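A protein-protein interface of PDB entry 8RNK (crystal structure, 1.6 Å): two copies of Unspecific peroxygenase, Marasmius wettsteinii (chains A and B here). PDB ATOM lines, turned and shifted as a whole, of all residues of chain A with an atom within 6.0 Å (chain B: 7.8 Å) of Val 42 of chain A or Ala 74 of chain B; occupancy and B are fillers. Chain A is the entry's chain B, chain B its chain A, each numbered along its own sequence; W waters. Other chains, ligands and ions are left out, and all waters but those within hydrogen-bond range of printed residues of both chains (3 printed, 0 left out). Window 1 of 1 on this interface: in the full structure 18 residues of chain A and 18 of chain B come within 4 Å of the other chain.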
ATOM      1  N   ILE A  40      25.020  -5.700   3.048  1.00  0.00           N
ATOM      2  CA  ILE A  40      26.094  -5.121   3.835  1.00  0.00           C
ATOM      3  C   ILE A  40      25.533  -3.973   4.679  1.00  0.00           C
ATOM      4  O   ILE A  40      24.943  -3.050   4.137  1.00  0.00           O
ATOM      5  CB  ILE A  40      27.218  -4.626   2.906  1.00  0.00           C
ATOM      6  CG1 ILE A  40      27.879  -5.813   2.194  1.00  0.00           C
ATOM      7  CG2 ILE A  40      28.218  -3.778   3.673  1.00  0.00           C
ATOM      8  CD1 ILE A  40      29.029  -5.464   1.308  1.00  0.00           C
ATOM      9  N   SER A  41      25.709  -4.109   5.994  1.00  0.00           N
ATOM     10  CA  SER A  41      25.190  -3.164   6.977  1.00  0.00           C
ATOM     11  C   SER A  41      26.307  -2.242   7.450  1.00  0.00           C
ATOM     12  O   SER A  41      27.488  -2.523   7.258  1.00  0.00           O
ATOM     13  CB  SER A  41      24.632  -3.913   8.141  1.00  0.00           C
ATOM     14  OG  SER A  41      25.676  -4.536   8.854  1.00  0.00           O
ATOM     15  N   VAL A  42      25.946  -1.179   8.186  1.00  0.00           N
ATOM     16  CA  VAL A  42      26.973  -0.302   8.715  1.00  0.00           C
ATOM     17  C   VAL A  42      27.821  -1.040   9.752  1.00  0.00           C
ATOM     18  O   VAL A  42      29.043  -0.915   9.765  1.00  0.00           O
ATOM     19  CB  VAL A  42      26.375   1.018   9.238  1.00  0.00           C
ATOM     20  CG1 VAL A  42      27.449   1.862   9.908  1.00  0.00           C
ATOM     21  CG2 VAL A  42      25.681   1.762   8.097  1.00  0.00           C
ATOM     22  N   PRO A  43      27.253  -1.845  10.679  1.00  0.00           N
ATOM     23  CA  PRO A  43      28.099  -2.600  11.601  1.00  0.00           C
ATOM     24  C   PRO A  43      29.118  -3.487  10.881  1.00  0.00           C
ATOM     25  O   PRO A  43      30.258  -3.573  11.327  1.00  0.00           O
ATOM     26  CB  PRO A  43      27.084  -3.398  12.438  1.00  0.00           C
ATOM     27  CG  PRO A  43      25.839  -2.503  12.395  1.00  0.00           C
ATOM     28  CD  PRO A  43      25.821  -1.965  10.983  1.00  0.00           C
ATOM     29  N   MET A  44      28.720  -4.079   9.750  1.00  0.00           N
ATOM     30  CA  MET A  44      29.643  -4.903   8.978  1.00  0.00           C
ATOM     31  C   MET A  44      30.786  -4.062   8.408  1.00  0.00           C
ATOM     32  O   MET A  44      31.955  -4.472   8.461  1.00  0.00           O
ATOM     33  CB  MET A  44      28.902  -5.636   7.863  1.00  0.00           C
ATOM     34  CG  MET A  44      28.059  -6.794   8.379  1.00  0.00           C
ATOM     35  SD  MET A  44      26.835  -7.263   7.170  1.00  0.00           S
ATOM     36  CE  MET A  44      27.873  -8.081   5.975  1.00  0.00           C
ATOM     37  N   ILE A  45      30.458  -2.863   7.890  1.00  0.00           N
ATOM     38  CA  ILE A  45      31.474  -1.957   7.365  1.00  0.00           C
ATOM     39  C   ILE A  45      32.440  -1.521   8.470  1.00  0.00           C
ATOM     40  O   ILE A  45      33.660  -1.489   8.267  1.00  0.00           O
ATOM     41  CB  ILE A  45      30.814  -0.757   6.664  1.00  0.00           C
ATOM     42  CG1 ILE A  45      30.115  -1.173   5.369  1.00  0.00           C
ATOM     43  CG2 ILE A  45      31.835   0.346   6.419  1.00  0.00           C
ATOM     44  CD1 ILE A  45      29.169  -0.145   4.794  1.00  0.00           C
ATOM     45  N   VAL A  46      31.904  -1.177   9.654  1.00  0.00           N
ATOM     46  CA  VAL A  46      32.719  -0.767  10.784  1.00  0.00           C
ATOM     47  C   VAL A  46      33.738  -1.849  11.141  1.00  0.00           C
ATOM     48  O   VAL A  46      34.927  -1.584  11.287  1.00  0.00           O
ATOM     49  CB  VAL A  46      31.844  -0.384  11.997  1.00  0.00           C
ATOM     50  CG1 VAL A  46      32.660  -0.202  13.253  1.00  0.00           C
ATOM     51  CG2 VAL A  46      31.026   0.870  11.705  1.00  0.00           C
ATOM     52  N   LYS A  47      33.263  -3.092  11.267  1.00  0.00           N
ATOM     53  CA  LYS A  47      34.141  -4.190  11.639  1.00  0.00           C
ATOM     54  C   LYS A  47      35.166  -4.455  10.527  1.00  0.00           C
ATOM     55  O   LYS A  47      36.353  -4.619  10.792  1.00  0.00           O
ATOM     56  CB  LYS A  47      33.289  -5.426  11.936  1.00  0.00           C
ATOM     57  CG  LYS A  47      34.089  -6.628  12.420  1.00  0.00           C
ATOM     58  CD  LYS A  47      33.226  -7.700  13.050  1.00  0.00           C
ATOM     59  CE  LYS A  47      34.030  -8.735  13.804  1.00  0.00           C
ATOM     60  NZ  LYS A  47      33.228  -9.376  14.877  1.00  0.00           N
ATOM     61  N   LEU A  60      33.458   5.599   9.666  1.00  0.00           N
ATOM     62  CA  LEU A  60      32.696   4.566   8.978  1.00  0.00           C
ATOM     63  C   LEU A  60      31.214   4.605   9.352  1.00  0.00           C
ATOM     64  O   LEU A  60      30.373   4.270   8.519  1.00  0.00           O
ATOM     65  CB  LEU A  60      33.312   3.191   9.247  1.00  0.00           C
ATOM     66  CG  LEU A  60      34.731   3.032   8.712  1.00  0.00           C
ATOM     67  CD1 LEU A  60      35.330   1.697   9.115  1.00  0.00           C
ATOM     68  CD2 LEU A  60      34.745   3.196   7.208  1.00  0.00           C
ATOM     69  N   ILE A  61      30.871   5.029  10.579  1.00  0.00           N
ATOM     70  CA  ILE A  61      29.464   5.228  10.905  1.00  0.00           C
ATOM     71  C   ILE A  61      28.892   6.395  10.103  1.00  0.00           C
ATOM     72  O   ILE A  61      27.792   6.295   9.555  1.00  0.00           O
ATOM     73  CB  ILE A  61      29.275   5.392  12.423  1.00  0.00           C
ATOM     74  CG1 ILE A  61      29.571   4.072  13.142  1.00  0.00           C
ATOM     75  CG2 ILE A  61      27.875   5.903  12.716  1.00  0.00           C
ATOM     76  CD1 ILE A  61      29.600   4.149  14.644  1.00  0.00           C
ATOM     77  N   GLY A  64      29.014   5.438   6.385  1.00  0.00           N
ATOM     78  CA  GLY A  64      28.216   4.239   6.207  1.00  0.00           C
ATOM     79  C   GLY A  64      26.721   4.543   6.176  1.00  0.00           C
ATOM     80  O   GLY A  64      26.001   4.038   5.324  1.00  0.00           O
ATOM     81  N   LYS A  65      26.229   5.361   7.130  1.00  0.00           N
ATOM     82  CA  LYS A  65      24.805   5.645   7.171  1.00  0.00           C
ATOM     83  C   LYS A  65      24.367   6.509   5.992  1.00  0.00           C
ATOM     84  O   LYS A  65      23.244   6.384   5.517  1.00  0.00           O
ATOM     85  CB  LYS A  65      24.432   6.262   8.517  1.00  0.00           C
ATOM     86  CG  LYS A  65      24.529   5.274   9.665  1.00  0.00           C
ATOM     87  CD  LYS A  65      23.951   5.783  10.973  1.00  0.00           C
ATOM     88  CE  LYS A  65      24.590   7.059  11.448  1.00  0.00           C
ATOM     89  NZ  LYS A  65      24.170   7.372  12.833  1.00  0.00           N
ATOM     90  N   MET A  68      23.990   4.055   3.212  1.00  0.00           N
ATOM     91  CA  MET A  68      22.779   3.245   3.325  1.00  0.00           C
ATOM     92  C   MET A  68      21.612   3.870   2.555  1.00  0.00           C
ATOM     93  O   MET A  68      20.699   3.164   2.134  1.00  0.00           O
ATOM     94  CB  MET A  68      22.341   3.053   4.783  1.00  0.00           C
ATOM     95  CG  MET A  68      23.261   2.233   5.642  1.00  0.00           C
ATOM     96  SD  MET A  68      23.456   0.485   5.088  1.00  0.00           S
ATOM     97  CE  MET A  68      25.170   0.487   4.569  1.00  0.00           C
ATOM     98  N   ASP A  75      18.350  -1.549   6.117  1.00  0.00           N
ATOM     99  CA  ASP A  75      19.596  -1.377   6.854  1.00  0.00           C
ATOM    100  C   ASP A  75      20.797  -2.042   6.180  1.00  0.00           C
ATOM    101  O   ASP A  75      21.807  -2.262   6.839  1.00  0.00           O
ATOM    102  CB  ASP A  75      19.467  -1.865   8.301  1.00  0.00           C
ATOM    103  CG  ASP A  75      19.285  -3.363   8.493  1.00  0.00           C
ATOM    104  OD1 ASP A  75      19.070  -4.073   7.490  1.00  0.00           O
ATOM    105  OD2 ASP A  75      19.330  -3.800   9.649  1.00  0.00           O
ATOM    106  N   MET B  68      18.258   7.987  10.790  1.00  0.00           N
ATOM    107  CA  MET B  68      19.393   7.317  11.391  1.00  0.00           C
ATOM    108  C   MET B  68      20.596   8.260  11.435  1.00  0.00           C
ATOM    109  O   MET B  68      21.465   8.092  12.295  1.00  0.00           O
ATOM    110  CB  MET B  68      19.788   6.040  10.638  1.00  0.00           C
ATOM    111  CG  MET B  68      18.785   4.889  10.760  1.00  0.00           C
ATOM    112  SD  MET B  68      18.481   4.246  12.450  1.00  0.00           S
ATOM    113  CE  MET B  68      16.796   4.794  12.702  1.00  0.00           C
ATOM    114  N   SER B  71      21.954  10.246  14.864  1.00  0.00           N
ATOM    115  CA  SER B  71      22.643   9.660  16.003  1.00  0.00           C
ATOM    116  C   SER B  71      24.119   9.458  15.675  1.00  0.00           C
ATOM    117  O   SER B  71      24.543   9.558  14.515  1.00  0.00           O
ATOM    118  CB  SER B  71      22.024   8.347  16.419  1.00  0.00           C
ATOM    119  OG  SER B  71      22.432   7.326  15.516  1.00  0.00           O
ATOM    120  N   ARG B  72      24.872   9.069  16.713  1.00  0.00           N
ATOM    121  CA  ARG B  72      26.268   8.675  16.579  1.00  0.00           C
ATOM    122  C   ARG B  72      26.416   7.149  16.497  1.00  0.00           C
ATOM    123  O   ARG B  72      27.543   6.653  16.446  1.00  0.00           O
ATOM    124  CB  ARG B  72      27.068   9.206  17.773  1.00  0.00           C
ATOM    125  CG  ARG B  72      27.188  10.725  17.780  1.00  0.00           C
ATOM    126  CD  ARG B  72      28.113  11.255  18.853  1.00  0.00           C
ATOM    127  NE  ARG B  72      28.417  12.652  18.573  1.00  0.00           N
ATOM    128  CZ  ARG B  72      27.616  13.673  18.841  1.00  0.00           C
ATOM    129  NH1 ARG B  72      26.482  13.488  19.494  1.00  0.00           N
ATOM    130  NH2 ARG B  72      27.986  14.899  18.499  1.00  0.00           N
ATOM    131  N   GLU B  73      25.303   6.408  16.502  1.00  0.00           N
ATOM    132  CA  GLU B  73      25.368   4.950  16.505  1.00  0.00           C
ATOM    133  C   GLU B  73      25.326   4.414  15.074  1.00  0.00           C
ATOM    134  O   GLU B  73      24.813   5.054  14.159  1.00  0.00           O
ATOM    135  CB  GLU B  73      24.247   4.348  17.361  1.00  0.00           C
ATOM    136  CG  GLU B  73      24.474   4.517  18.850  1.00  0.00           C
ATOM    137  CD  GLU B  73      24.217   5.918  19.377  1.00  0.00           C
ATOM    138  OE1 GLU B  73      23.075   6.418  19.185  1.00  0.00           O
ATOM    139  OE2 GLU B  73      25.148   6.495  19.989  1.00  0.00           O
ATOM    140  N   ALA B  74      25.814   3.182  14.910  1.00  0.00           N
ATOM    141  CA  ALA B  74      25.907   2.536  13.613  1.00  0.00           C
ATOM    142  C   ALA B  74      24.554   2.305  12.931  1.00  0.00           C
ATOM    143  O   ALA B  74      24.480   2.451  11.712  1.00  0.00           O
ATOM    144  CB  ALA B  74      26.662   1.227  13.782  1.00  0.00           C
ATOM    145  N   ASP B  75      23.494   1.924  13.682  1.00  0.00           N
ATOM    146  CA  ASP B  75      22.237   1.558  13.050  1.00  0.00           C
ATOM    147  C   ASP B  75      21.017   1.762  13.949  1.00  0.00           C
ATOM    148  O   ASP B  75      19.963   1.190  13.694  1.00  0.00           O
ATOM    149  CB  ASP B  75      22.258   0.108  12.562  1.00  0.00           C
ATOM    150  CG  ASP B  75      22.337  -0.972  13.626  1.00  0.00           C
ATOM    151  OD1 ASP B  75      22.513  -0.651  14.818  1.00  0.00           O
ATOM    152  OD2 ASP B  75      22.221  -2.144  13.231  1.00  0.00           O
ATOM    153  N   THR B  76      21.122   2.647  14.942  1.00  0.00           N
ATOM    154  CA  THR B  76      20.001   2.907  15.822  1.00  0.00           C
ATOM    155  C   THR B  76      19.992   4.386  16.187  1.00  0.00           C
ATOM    156  O   THR B  76      20.999   5.060  16.033  1.00  0.00           O
ATOM    157  CB  THR B  76      20.036   2.104  17.132  1.00  0.00           C
ATOM    158  OG1 THR B  76      21.230   2.360  17.860  1.00  0.00           O
ATOM    159  CG2 THR B  76      19.870   0.619  16.906  1.00  0.00           C
ATOM    160  N   ILE B  77      18.827   4.833  16.639  1.00  0.00           N
ATOM    161  CA  ILE B  77      18.659   6.146  17.243  1.00  0.00           C
ATOM    162  C   ILE B  77      17.950   6.017  18.588  1.00  0.00           C
ATOM    163  O   ILE B  77      17.327   4.999  18.881  1.00  0.00           O
ATOM    164  CB  ILE B  77      17.809   7.054  16.324  1.00  0.00           C
ATOM    165  CG1 ILE B  77      16.402   6.479  16.113  1.00  0.00           C
ATOM    166  CG2 ILE B  77      18.526   7.314  15.013  1.00  0.00           C
ATOM    167  CD1 ILE B  77      15.413   7.426  15.480  1.00  0.00           C
HETATM  168  O   HOH W   1      25.627   9.939  11.679  1.00  0.00           O
HETATM  169  O   HOH W   2      19.317  -2.159  11.615  1.00  0.00           O
HETATM  170  O   HOH W   3      22.239  -2.765  10.725  1.00  0.00           O
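No residue of chain B comes within 4 Å of Ser 41 of chain A.
Val 42 of chain A touches just one residue of chain B: Ala 74.
Pro 43 of chain A touches just one residue of chain B: Asp 75 (3.7 Å).
Of the printed residues of chain B, Lys 65 of chain A touches Met 68, Ser 71, Glu 73 and Ala 74.
Of the printed residues of chain A, Met 68 of chain B touches Lys 65 (2.9 Å).
Of the printed residues of chain A, Ser 71 of chain B touches Lys 65 (2.8 Å).
Of the printed residues of chain A, Glu 73 of chain B touches Ile 61 and Lys 65.
Of chain A, only Val 42 (3.4 Å), Ile 61 (3.9 Å) and Lys 65 (3.5 Å) come within 4 Å of Ala 74 of chain B.
Printed residues of chain A within 4 Å of Asp 75 of chain B: Pro 43 (3.7 Å).
The nearest residue of chain A that does not touch Ala 74 of chain B is Pro 43 of chain A (4.1 Å).
The side-chain hydroxyl (OG) of Ser 71 of chain B lies within hydrogen-bond range of the backbone carbonyl oxygen (O) of Met 68 of chain B, at 3.4 Å.
The backbone NH of Glu 73 of chain B sits at hydrogen-bond distance from the side-chain hydroxyl of Ser 71 of chain B.
The side-chain hydroxyl of Ser 71 of chain B sits at hydrogen-bond distance from the backbone carbonyl oxygen of Thr 76 of chain B, at 2.7 Å.
Positions printed for both chains: 68 and 75.
Of the 9 pairs that touch across the chains among the printed residues, none has its exchanged pair printed and touching as well.
Water W2 bridges the side-chain carboxylate of Asp 75 of chain A (2.6 Å) and the side-chain carboxylate of Asp 75 of chain B (3.3 Å).
Water W3 lies within hydrogen-bond range of OD2 of Asp 75 of chain B (2.6 Å) and OD2 of Asp 75 of chain A (3.3 Å).
Water W1 lies within hydrogen-bond range of the backbone carbonyl oxygen (O) of Ser 71 of chain B (3.1 Å) and the side-chain amino group (NZ) of Lys 65 of chain A (3.2 Å).
Printed residues of chain B that touch a printed residue of chain A: Met 68, Ser 71, Arg 72, Glu 73, Ala 74 and Asp 75.
Hydrophobic or aromatic side chains of chain A that line the printed part of chain B: Val 42, Pro 43 and Ile 61.
Among the printed residues, 9 pairs touch across the chains.
Among the printed residues, no Asp or Glu carboxylate lies within 4 Å of a Lys or Arg side-chain nitrogen of the other chain.
Val 42 of chain A touches Ala 74 of chain B (CB to O, 3.4 Å).
CG of Pro 43 of chain A touches OD2 of Asp 75 of chain B (3.7 Å).
O of Arg 72 of chain B touches CD1 of Ile 61 of chain A (3.7 Å).
Ile 61 of chain A touches Glu 73 of chain B.
Ile 61 of chain A touches Ala 74 of chain B.
Lys 65 of chain A touches Ala 74 of chain B.
The backbone carbonyl oxygen (O) of Met 68 of chain B sits at hydrogen-bond distance from the side-chain amino group (NZ) of Lys 65 of chain A (2.9 Å).
O of Ser 71 of chain B is in hydrogen-bond range of NZ of Lys 65 of chain A, 2.8 Å away.
The backbone carbonyl oxygen (O) of Glu 73 of chain B sits at hydrogen-bond distance from the side-chain amino group (NZ) of Lys 65 of chain A.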
